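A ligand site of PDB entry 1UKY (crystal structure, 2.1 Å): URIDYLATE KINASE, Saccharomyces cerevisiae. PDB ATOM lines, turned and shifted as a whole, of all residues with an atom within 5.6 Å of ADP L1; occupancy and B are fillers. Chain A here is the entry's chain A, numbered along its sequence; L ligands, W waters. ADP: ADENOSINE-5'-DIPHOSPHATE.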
ATOM      1  N   GLY A  22       9.788   4.360  14.741  1.00  0.00           N
ATOM      2  CA  GLY A  22       9.822   5.619  15.479  1.00  0.00           C
ATOM      3  C   GLY A  22       8.568   5.909  16.324  1.00  0.00           C
ATOM      4  O   GLY A  22       7.511   5.331  16.154  1.00  0.00           O
ATOM      5  N   GLY A  23       8.623   6.835  17.273  1.00  0.00           N
ATOM      6  CA  GLY A  23       7.525   7.095  18.164  1.00  0.00           C
ATOM      7  C   GLY A  23       6.455   7.854  17.448  1.00  0.00           C
ATOM      8  O   GLY A  23       6.630   8.321  16.322  1.00  0.00           O
ATOM      9  N   PRO A  24       5.339   8.048  18.136  1.00  0.00           N
ATOM     10  CA  PRO A  24       4.195   8.696  17.516  1.00  0.00           C
ATOM     11  C   PRO A  24       4.524  10.132  17.111  1.00  0.00           C
ATOM     12  O   PRO A  24       5.056  10.838  17.985  1.00  0.00           O
ATOM     13  CB  PRO A  24       3.116   8.526  18.591  1.00  0.00           C
ATOM     14  CG  PRO A  24       3.820   8.338  19.908  1.00  0.00           C
ATOM     15  CD  PRO A  24       5.052   7.534  19.470  1.00  0.00           C
ATOM     16  N   GLY A  25       4.273  10.638  15.884  1.00  0.00           N
ATOM     17  CA  GLY A  25       4.539  12.030  15.545  1.00  0.00           C
ATOM     18  C   GLY A  25       5.994  12.289  15.169  1.00  0.00           C
ATOM     19  O   GLY A  25       6.397  13.439  15.088  1.00  0.00           O
ATOM     20  N   ALA A  26       6.804  11.258  14.921  1.00  0.00           N
ATOM     21  CA  ALA A  26       8.194  11.383  14.624  1.00  0.00           C
ATOM     22  C   ALA A  26       8.377  11.704  13.175  1.00  0.00           C
ATOM     23  O   ALA A  26       9.525  12.032  12.827  1.00  0.00           O
ATOM     24  CB  ALA A  26       8.985  10.103  14.836  1.00  0.00           C
ATOM     25  N   GLY A  27       7.354  11.553  12.338  1.00  0.00           N
ATOM     26  CA  GLY A  27       7.420  11.934  10.940  1.00  0.00           C
ATOM     27  C   GLY A  27       7.412  10.746   9.999  1.00  0.00           C
ATOM     28  O   GLY A  27       7.725  10.969   8.819  1.00  0.00           O
ATOM     29  N   LYS A  28       7.039   9.517  10.415  1.00  0.00           N
ATOM     30  CA  LYS A  28       7.095   8.300   9.590  1.00  0.00           C
ATOM     31  C   LYS A  28       6.174   8.433   8.410  1.00  0.00           C
ATOM     32  O   LYS A  28       6.607   8.328   7.258  1.00  0.00           O
ATOM     33  CB  LYS A  28       6.662   7.124  10.392  1.00  0.00           C
ATOM     34  CG  LYS A  28       7.564   6.948  11.628  1.00  0.00           C
ATOM     35  CD  LYS A  28       7.203   5.731  12.426  1.00  0.00           C
ATOM     36  CE  LYS A  28       5.749   5.765  12.841  1.00  0.00           C
ATOM     37  NZ  LYS A  28       5.538   6.783  13.864  1.00  0.00           N
ATOM     38  N   GLY A  29       4.932   8.810   8.667  1.00  0.00           N
ATOM     39  CA  GLY A  29       3.950   9.018   7.627  1.00  0.00           C
ATOM     40  C   GLY A  29       4.411  10.049   6.655  1.00  0.00           C
ATOM     41  O   GLY A  29       4.396   9.859   5.439  1.00  0.00           O
ATOM     42  N   THR A  30       4.871  11.158   7.167  1.00  0.00           N
ATOM     43  CA  THR A  30       5.394  12.213   6.293  1.00  0.00           C
ATOM     44  C   THR A  30       6.548  11.800   5.364  1.00  0.00           C
ATOM     45  O   THR A  30       6.542  12.053   4.145  1.00  0.00           O
ATOM     46  CB  THR A  30       5.819  13.446   7.181  1.00  0.00           C
ATOM     47  OG1 THR A  30       4.587  13.878   7.712  1.00  0.00           O
ATOM     48  CG2 THR A  30       6.419  14.669   6.455  1.00  0.00           C
ATOM     49  N   GLN A  31       7.567  11.114   5.856  1.00  0.00           N
ATOM     50  CA  GLN A  31       8.703  10.774   5.048  1.00  0.00           C
ATOM     51  C   GLN A  31       8.378   9.717   4.014  1.00  0.00           C
ATOM     52  O   GLN A  31       8.853   9.795   2.876  1.00  0.00           O
ATOM     53  CB  GLN A  31       9.851  10.343   5.980  1.00  0.00           C
ATOM     54  CG  GLN A  31      10.415  11.632   6.720  1.00  0.00           C
ATOM     55  CD  GLN A  31      10.857  12.783   5.791  1.00  0.00           C
ATOM     56  OE1 GLN A  31      10.634  13.975   5.991  1.00  0.00           O
ATOM     57  NE2 GLN A  31      11.503  12.503   4.696  1.00  0.00           N
ATOM     58  N   ASP A 102       5.417   1.029   7.426  1.00  0.00           N
ATOM     59  CA  ASP A 102       5.524   2.061   8.400  1.00  0.00           C
ATOM     60  C   ASP A 102       4.794   1.650   9.685  1.00  0.00           C
ATOM     61  O   ASP A 102       3.624   1.229   9.592  1.00  0.00           O
ATOM     62  CB  ASP A 102       4.947   3.201   7.604  1.00  0.00           C
ATOM     63  CG  ASP A 102       4.250   4.338   8.303  1.00  0.00           C
ATOM     64  OD1 ASP A 102       4.379   4.517   9.511  1.00  0.00           O
ATOM     65  OD2 ASP A 102       3.570   5.080   7.603  1.00  0.00           O
ATOM     66  N   ARG A 137       4.420  18.152  17.765  1.00  0.00           N
ATOM     67  CA  ARG A 137       3.856  17.719  16.468  1.00  0.00           C
ATOM     68  C   ARG A 137       2.506  17.005  16.628  1.00  0.00           C
ATOM     69  O   ARG A 137       1.586  17.230  15.838  1.00  0.00           O
ATOM     70  CB  ARG A 137       4.813  16.775  15.734  1.00  0.00           C
ATOM     71  CG  ARG A 137       6.018  17.572  15.298  1.00  0.00           C
ATOM     72  CD  ARG A 137       6.960  16.659  14.590  1.00  0.00           C
ATOM     73  NE  ARG A 137       8.176  17.371  14.308  1.00  0.00           N
ATOM     74  CZ  ARG A 137       9.259  16.754  13.822  1.00  0.00           C
ATOM     75  NH1 ARG A 137       9.253  15.440  13.587  1.00  0.00           N
ATOM     76  NH2 ARG A 137      10.376  17.458  13.611  1.00  0.00           N
ATOM     77  N   LEU A 138       2.263  16.160  17.636  1.00  0.00           N
ATOM     78  CA  LEU A 138       0.982  15.505  17.788  1.00  0.00           C
ATOM     79  C   LEU A 138      -0.067  16.473  18.275  1.00  0.00           C
ATOM     80  O   LEU A 138      -1.207  16.353  17.876  1.00  0.00           O
ATOM     81  CB  LEU A 138       1.106  14.356  18.763  1.00  0.00           C
ATOM     82  CG  LEU A 138       1.835  13.096  18.284  1.00  0.00           C
ATOM     83  CD1 LEU A 138       1.846  12.090  19.439  1.00  0.00           C
ATOM     84  CD2 LEU A 138       1.146  12.436  17.089  1.00  0.00           C
ATOM     85  N   GLU A 140      -0.284  19.732  17.480  1.00  0.00           N
ATOM     86  CA  GLU A 140      -0.648  20.400  16.269  1.00  0.00           C
ATOM     87  C   GLU A 140      -1.368  19.469  15.285  1.00  0.00           C
ATOM     88  O   GLU A 140      -2.364  19.947  14.731  1.00  0.00           O
ATOM     89  CB  GLU A 140       0.580  21.008  15.608  1.00  0.00           C
ATOM     90  CG  GLU A 140       0.669  22.521  15.958  1.00  0.00           C
ATOM     91  CD  GLU A 140      -0.585  23.396  15.657  1.00  0.00           C
ATOM     92  OE1 GLU A 140      -1.070  23.401  14.500  1.00  0.00           O
ATOM     93  OE2 GLU A 140      -1.072  24.080  16.575  1.00  0.00           O
ATOM     94  N   ARG A 141      -1.021  18.162  15.092  1.00  0.00           N
ATOM     95  CA  ARG A 141      -1.734  17.238  14.207  1.00  0.00           C
ATOM     96  C   ARG A 141      -3.158  17.065  14.723  1.00  0.00           C
ATOM     97  O   ARG A 141      -4.102  17.025  13.931  1.00  0.00           O
ATOM     98  CB  ARG A 141      -1.081  15.889  14.176  1.00  0.00           C
ATOM     99  CG  ARG A 141      -1.533  15.165  12.911  1.00  0.00           C
ATOM    100  CD  ARG A 141      -0.734  13.897  12.758  1.00  0.00           C
ATOM    101  NE  ARG A 141      -1.134  12.924  13.763  1.00  0.00           N
ATOM    102  CZ  ARG A 141      -0.429  11.817  14.060  1.00  0.00           C
ATOM    103  NH1 ARG A 141       0.697  11.527  13.447  1.00  0.00           N
ATOM    104  NH2 ARG A 141      -0.847  10.945  14.980  1.00  0.00           N
ATOM    105  N   ARG A 158       0.336   6.359  24.380  1.00  0.00           N
ATOM    106  CA  ARG A 158       1.161   6.039  23.202  1.00  0.00           C
ATOM    107  C   ARG A 158       2.665   6.271  23.467  1.00  0.00           C
ATOM    108  O   ARG A 158       3.503   5.417  23.103  1.00  0.00           O
ATOM    109  CB  ARG A 158       0.654   6.889  22.054  1.00  0.00           C
ATOM    110  CG  ARG A 158      -0.730   6.523  21.618  1.00  0.00           C
ATOM    111  CD  ARG A 158      -1.329   7.681  20.900  1.00  0.00           C
ATOM    112  NE  ARG A 158      -0.690   7.892  19.644  1.00  0.00           N
ATOM    113  CZ  ARG A 158      -0.988   8.956  18.881  1.00  0.00           C
ATOM    114  NH1 ARG A 158      -1.864   9.861  19.268  1.00  0.00           N
ATOM    115  NH2 ARG A 158      -0.507   9.070  17.647  1.00  0.00           N
ATOM    116  N   CYS A 184      14.726  13.120  13.763  1.00  0.00           N
ATOM    117  CA  CYS A 184      13.463  13.712  13.342  1.00  0.00           C
ATOM    118  C   CYS A 184      13.410  15.251  13.413  1.00  0.00           C
ATOM    119  O   CYS A 184      12.658  16.001  12.792  1.00  0.00           O
ATOM    120  CB  CYS A 184      12.403  13.101  14.227  1.00  0.00           C
ATOM    121  SG  CYS A 184      12.453  13.940  15.815  1.00  0.00           S
ATOM    122  N   ARG A 186      14.564  18.096  12.369  1.00  0.00           N
ATOM    123  CA  ARG A 186      14.999  19.084  11.403  1.00  0.00           C
ATOM    124  C   ARG A 186      13.786  19.380  10.550  1.00  0.00           C
ATOM    125  O   ARG A 186      12.712  18.818  10.792  1.00  0.00           O
ATOM    126  CB  ARG A 186      16.117  18.519  10.525  1.00  0.00           C
ATOM    127  CG  ARG A 186      17.386  18.243  11.305  1.00  0.00           C
ATOM    128  CD  ARG A 186      18.465  17.768  10.324  1.00  0.00           C
ATOM    129  NE  ARG A 186      18.933  16.417  10.634  1.00  0.00           N
ATOM    130  CZ  ARG A 186      18.246  15.310  10.301  1.00  0.00           C
ATOM    131  NH1 ARG A 186      17.087  15.324   9.651  1.00  0.00           N
ATOM    132  NH2 ARG A 186      18.778  14.123  10.538  1.00  0.00           N
ATOM    133  N   SER A 187      13.851  20.254   9.546  1.00  0.00           N
ATOM    134  CA  SER A 187      12.695  20.531   8.737  1.00  0.00           C
ATOM    135  C   SER A 187      12.385  19.269   7.915  1.00  0.00           C
ATOM    136  O   SER A 187      13.232  18.357   7.782  1.00  0.00           O
ATOM    137  CB  SER A 187      12.999  21.755   7.816  1.00  0.00           C
ATOM    138  OG  SER A 187      13.971  21.460   6.818  1.00  0.00           O
ATOM    139  N   VAL A 188      11.172  19.222   7.354  1.00  0.00           N
ATOM    140  CA  VAL A 188      10.757  18.100   6.541  1.00  0.00           C
ATOM    141  C   VAL A 188      11.797  17.879   5.442  1.00  0.00           C
ATOM    142  O   VAL A 188      12.279  16.748   5.245  1.00  0.00           O
ATOM    143  CB  VAL A 188       9.382  18.358   5.914  1.00  0.00           C
ATOM    144  CG1 VAL A 188       8.983  17.197   5.026  1.00  0.00           C
ATOM    145  CG2 VAL A 188       8.334  18.431   6.984  1.00  0.00           C
ATOM    146  N   VAL A 191      15.112  16.562   6.877  1.00  0.00           N
ATOM    147  CA  VAL A 191      15.045  15.143   7.272  1.00  0.00           C
ATOM    148  C   VAL A 191      15.014  14.340   5.973  1.00  0.00           C
ATOM    149  O   VAL A 191      15.750  13.376   5.816  1.00  0.00           O
ATOM    150  CB  VAL A 191      13.786  14.869   8.077  1.00  0.00           C
ATOM    151  CG1 VAL A 191      13.842  13.405   8.470  1.00  0.00           C
ATOM    152  CG2 VAL A 191      13.740  15.648   9.379  1.00  0.00           C
HETATM  153  PB  ADP L   1       4.096   9.644  12.368  1.00  0.00           P
HETATM  154  O1B ADP L   1       3.577   8.980  11.195  1.00  0.00           O
HETATM  155  O2B ADP L   1       5.406   9.272  12.818  1.00  0.00           O
HETATM  156  O3B ADP L   1       3.199   9.650  13.570  1.00  0.00           O
HETATM  157  PA  ADP L   1       3.607  12.222  10.951  1.00  0.00           P
HETATM  158  O1A ADP L   1       2.159  12.328  10.831  1.00  0.00           O
HETATM  159  O2A ADP L   1       4.305  12.064   9.698  1.00  0.00           O
HETATM  160  O3A ADP L   1       4.118  11.125  11.922  1.00  0.00           O
HETATM  161  O5' ADP L   1       4.111  13.598  11.516  1.00  0.00           O
HETATM  162  C5' ADP L   1       3.558  14.164  12.733  1.00  0.00           C
HETATM  163  C4' ADP L   1       3.001  15.587  12.553  1.00  0.00           C
HETATM  164  O4' ADP L   1       4.026  16.611  12.456  1.00  0.00           O
HETATM  165  C3' ADP L   1       2.135  15.749  11.258  1.00  0.00           C
HETATM  166  O3' ADP L   1       1.203  16.840  11.415  1.00  0.00           O
HETATM  167  C2' ADP L   1       3.206  16.120  10.185  1.00  0.00           C
HETATM  168  O2' ADP L   1       2.739  17.164   9.333  1.00  0.00           O
HETATM  169  C1' ADP L   1       4.343  16.584  11.079  1.00  0.00           C
HETATM  170  N9  ADP L   1       5.679  16.684  10.634  1.00  0.00           N
HETATM  171  C8  ADP L   1       6.342  15.639  10.083  1.00  0.00           C
HETATM  172  N7  ADP L   1       7.605  15.904   9.957  1.00  0.00           N
HETATM  173  C5  ADP L   1       7.824  17.176  10.433  1.00  0.00           C
HETATM  174  C6  ADP L   1       8.992  17.975  10.562  1.00  0.00           C
HETATM  175  N6  ADP L   1      10.220  17.584  10.217  1.00  0.00           N
HETATM  176  N1  ADP L   1       8.796  19.171  11.085  1.00  0.00           N
HETATM  177  C2  ADP L   1       7.541  19.519  11.437  1.00  0.00           C
HETATM  178  N3  ADP L   1       6.371  18.910  11.381  1.00  0.00           N
HETATM  179  C4  ADP L   1       6.561  17.690  10.851  1.00  0.00           C
HETATM  180  PB  ADP L   2       1.413   6.976  15.098  1.00  0.00           P
HETATM  181  O1B ADP L   2       1.252   7.124  16.520  1.00  0.00           O
HETATM  182  O2B ADP L   2       2.675   6.468  14.618  1.00  0.00           O
HETATM  183  O3B ADP L   2       1.060   8.302  14.480  1.00  0.00           O
HETATM  184  PA  ADP L   2      -0.371   4.978  13.923  1.00  0.00           P
HETATM  185  O1A ADP L   2      -1.464   5.593  13.207  1.00  0.00           O
HETATM  186  O2A ADP L   2       0.572   4.188  13.218  1.00  0.00           O
HETATM  187  O3A ADP L   2       0.266   6.037  14.777  1.00  0.00           O
HETATM  188  O5' ADP L   2      -1.008   3.912  14.949  1.00  0.00           O
HETATM  189  C5' ADP L   2      -2.104   4.299  15.781  1.00  0.00           C
HETATM  190  C4' ADP L   2      -2.498   3.194  16.765  1.00  0.00           C
HETATM  191  O4' ADP L   2      -2.874   1.962  16.120  1.00  0.00           O
HETATM  192  C3' ADP L   2      -1.324   2.806  17.691  1.00  0.00           C
HETATM  193  O3' ADP L   2      -1.254   3.697  18.786  1.00  0.00           O
HETATM  194  C2' ADP L   2      -1.690   1.411  18.141  1.00  0.00           C
HETATM  195  O2' ADP L   2      -2.831   1.534  18.940  1.00  0.00           O
HETATM  196  C1' ADP L   2      -1.974   1.070  16.702  1.00  0.00           C
HETATM  197  N9  ADP L   2      -1.094   0.273  15.926  1.00  0.00           N
HETATM  198  C8  ADP L   2      -0.273   0.852  14.982  1.00  0.00           C
HETATM  199  N7  ADP L   2       0.635   0.009  14.567  1.00  0.00           N
HETATM  200  C5  ADP L   2       0.459  -1.190  15.232  1.00  0.00           C
HETATM  201  C6  ADP L   2       1.175  -2.367  15.187  1.00  0.00           C
HETATM  202  N6  ADP L   2       2.274  -2.502  14.419  1.00  0.00           N
HETATM  203  N1  ADP L   2       0.699  -3.353  15.980  1.00  0.00           N
HETATM  204  C2  ADP L   2      -0.383  -3.126  16.735  1.00  0.00           C
HETATM  205  N3  ADP L   2      -1.152  -2.063  16.898  1.00  0.00           N
HETATM  206  C4  ADP L   2      -0.683  -1.057  16.101  1.00  0.00           C
HETATM  207  O   HOH W   1       2.316  15.387   7.058  1.00  0.00           O
HETATM  208  O   HOH W   2      10.014  14.787   9.081  1.00  0.00           O
HETATM  209  O   HOH W   3      10.629  21.564  11.760  1.00  0.00           O
HETATM  210  O   HOH W   4      -0.939  15.761   9.922  1.00  0.00           O
HETATM  211  O   HOH W   5       2.480   6.572  10.883  1.00  0.00           O
HETATM  212  O   HOH W   6       1.049   9.440   9.931  1.00  0.00           O
HETATM  213  O   HOH W   7       2.102  18.961  13.109  1.00  0.00           O
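The side-chain amino group (NZ) of Lys 28 lies within salt-bridge range of an oxygen (O2B) of ADP L2.
The backbone NH (N) of Thr 30 sits at hydrogen-bond distance from an oxygen (O2A) of ADP L1, 2.7 Å away.
The side-chain hydroxyl (OG1) of Thr 30 sits at hydrogen-bond distance from an oxygen (O2A) of ADP L1 (2.7 Å).
An oxygen (O2B) of ADP L1 sits at hydrogen-bond distance from the backbone NH of Ala 26 (3.2 Å).
An oxygen (O1B) of ADP L1 lies within hydrogen-bond range of the backbone NH of Gly 29 (2.9 Å).
The backbone NH of Gly 27 is in hydrogen-bond range of an oxygen (O2B) of ADP L1.
The guanidinium group (NH2) of Arg 137 lies close to a nitrogen (N1) of ADP L1, 3.4 Å away.
The backbone carbonyl oxygen (O) of Arg 186 is in hydrogen-bond range of a nitrogen (N6) of ADP L1, 2.8 Å away.
N of Lys 28 sits at hydrogen-bond distance from O2B of ADP L1 (2.9 Å).
The guanidinium group (NH2) of Arg 158 is in salt-bridge range of an oxygen (O1B) of ADP L2 (2.9 Å).
O3B of ADP L2 lies within salt-bridge range of NH2 of Arg 141, 3.3 Å away.
N of Gly 25 sits at hydrogen-bond distance from O3B of ADP L1, at 2.7 Å.
The side-chain amino group of Lys 28 is in salt-bridge range of an oxygen (O2B) of ADP L1 (2.7 Å).
The guanidinium group (NH1) of Arg 141 lies within salt-bridge range of an oxygen (O1A) of ADP L1.
Water W5 bridges an oxygen (O1B) of ADP L1 (2.7 Å) and the side-chain carboxylate of Asp 102 (3.1 Å).
Water W2 bridges a nitrogen (N7) of ADP L1 (2.8 Å) and the side-chain amide oxygen of Gln 31 (3.3 Å).
Water W7 lies within hydrogen-bond range of O3' of ADP L1 (2.9 Å) and O of Arg 137 (3.3 Å).
Water W1 bridges OG1 of Thr 30 and O2' of ADP L1.
NH2 of Arg 137 lies within hydrogen-bond range of O of Cys 184 (2.8 Å).
O of Val 188 sits close to OE1 of Gln 31, 3.3 Å away.
The side-chain amino group (NZ) of Lys 28 sits at hydrogen-bond distance from the backbone carbonyl oxygen (O) of Gly 23 (3.1 Å).
The side-chain amino group (NZ) of Lys 28 is in hydrogen-bond range of the backbone carbonyl oxygen (O) of Gly 22, at 3.4 Å.
An oxygen (O3B) of ADP L1 sits close to an oxygen (O3B) of ADP L2.
N of Val 188 sits close to N6 of ADP L1, 3.4 Å away.
Residues that only touch ADP L1: Gly 23 (3.8 Å), Pro 24 (3.8 Å), Cys 184 (3.9 Å) and Ser 187 (3.6 Å).
Hydrophobic or aromatic side chains that line ADP L1: Val 188.
14 residues have an atom within 4 Å of ADP L1: Gly 23, Pro 24, Gly 25, Ala 26, Gly 27, Lys 28, Gly 29, Thr 30, Arg 137, Arg 141, Cys 184, Arg 186, Ser 187 and Val 188.
Along chain A the residues within 4 Å of ADP L1 span positions 23 to 188.
The nearest printed residue that does not touch ADP L1 is Val 191 (4.1 Å).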
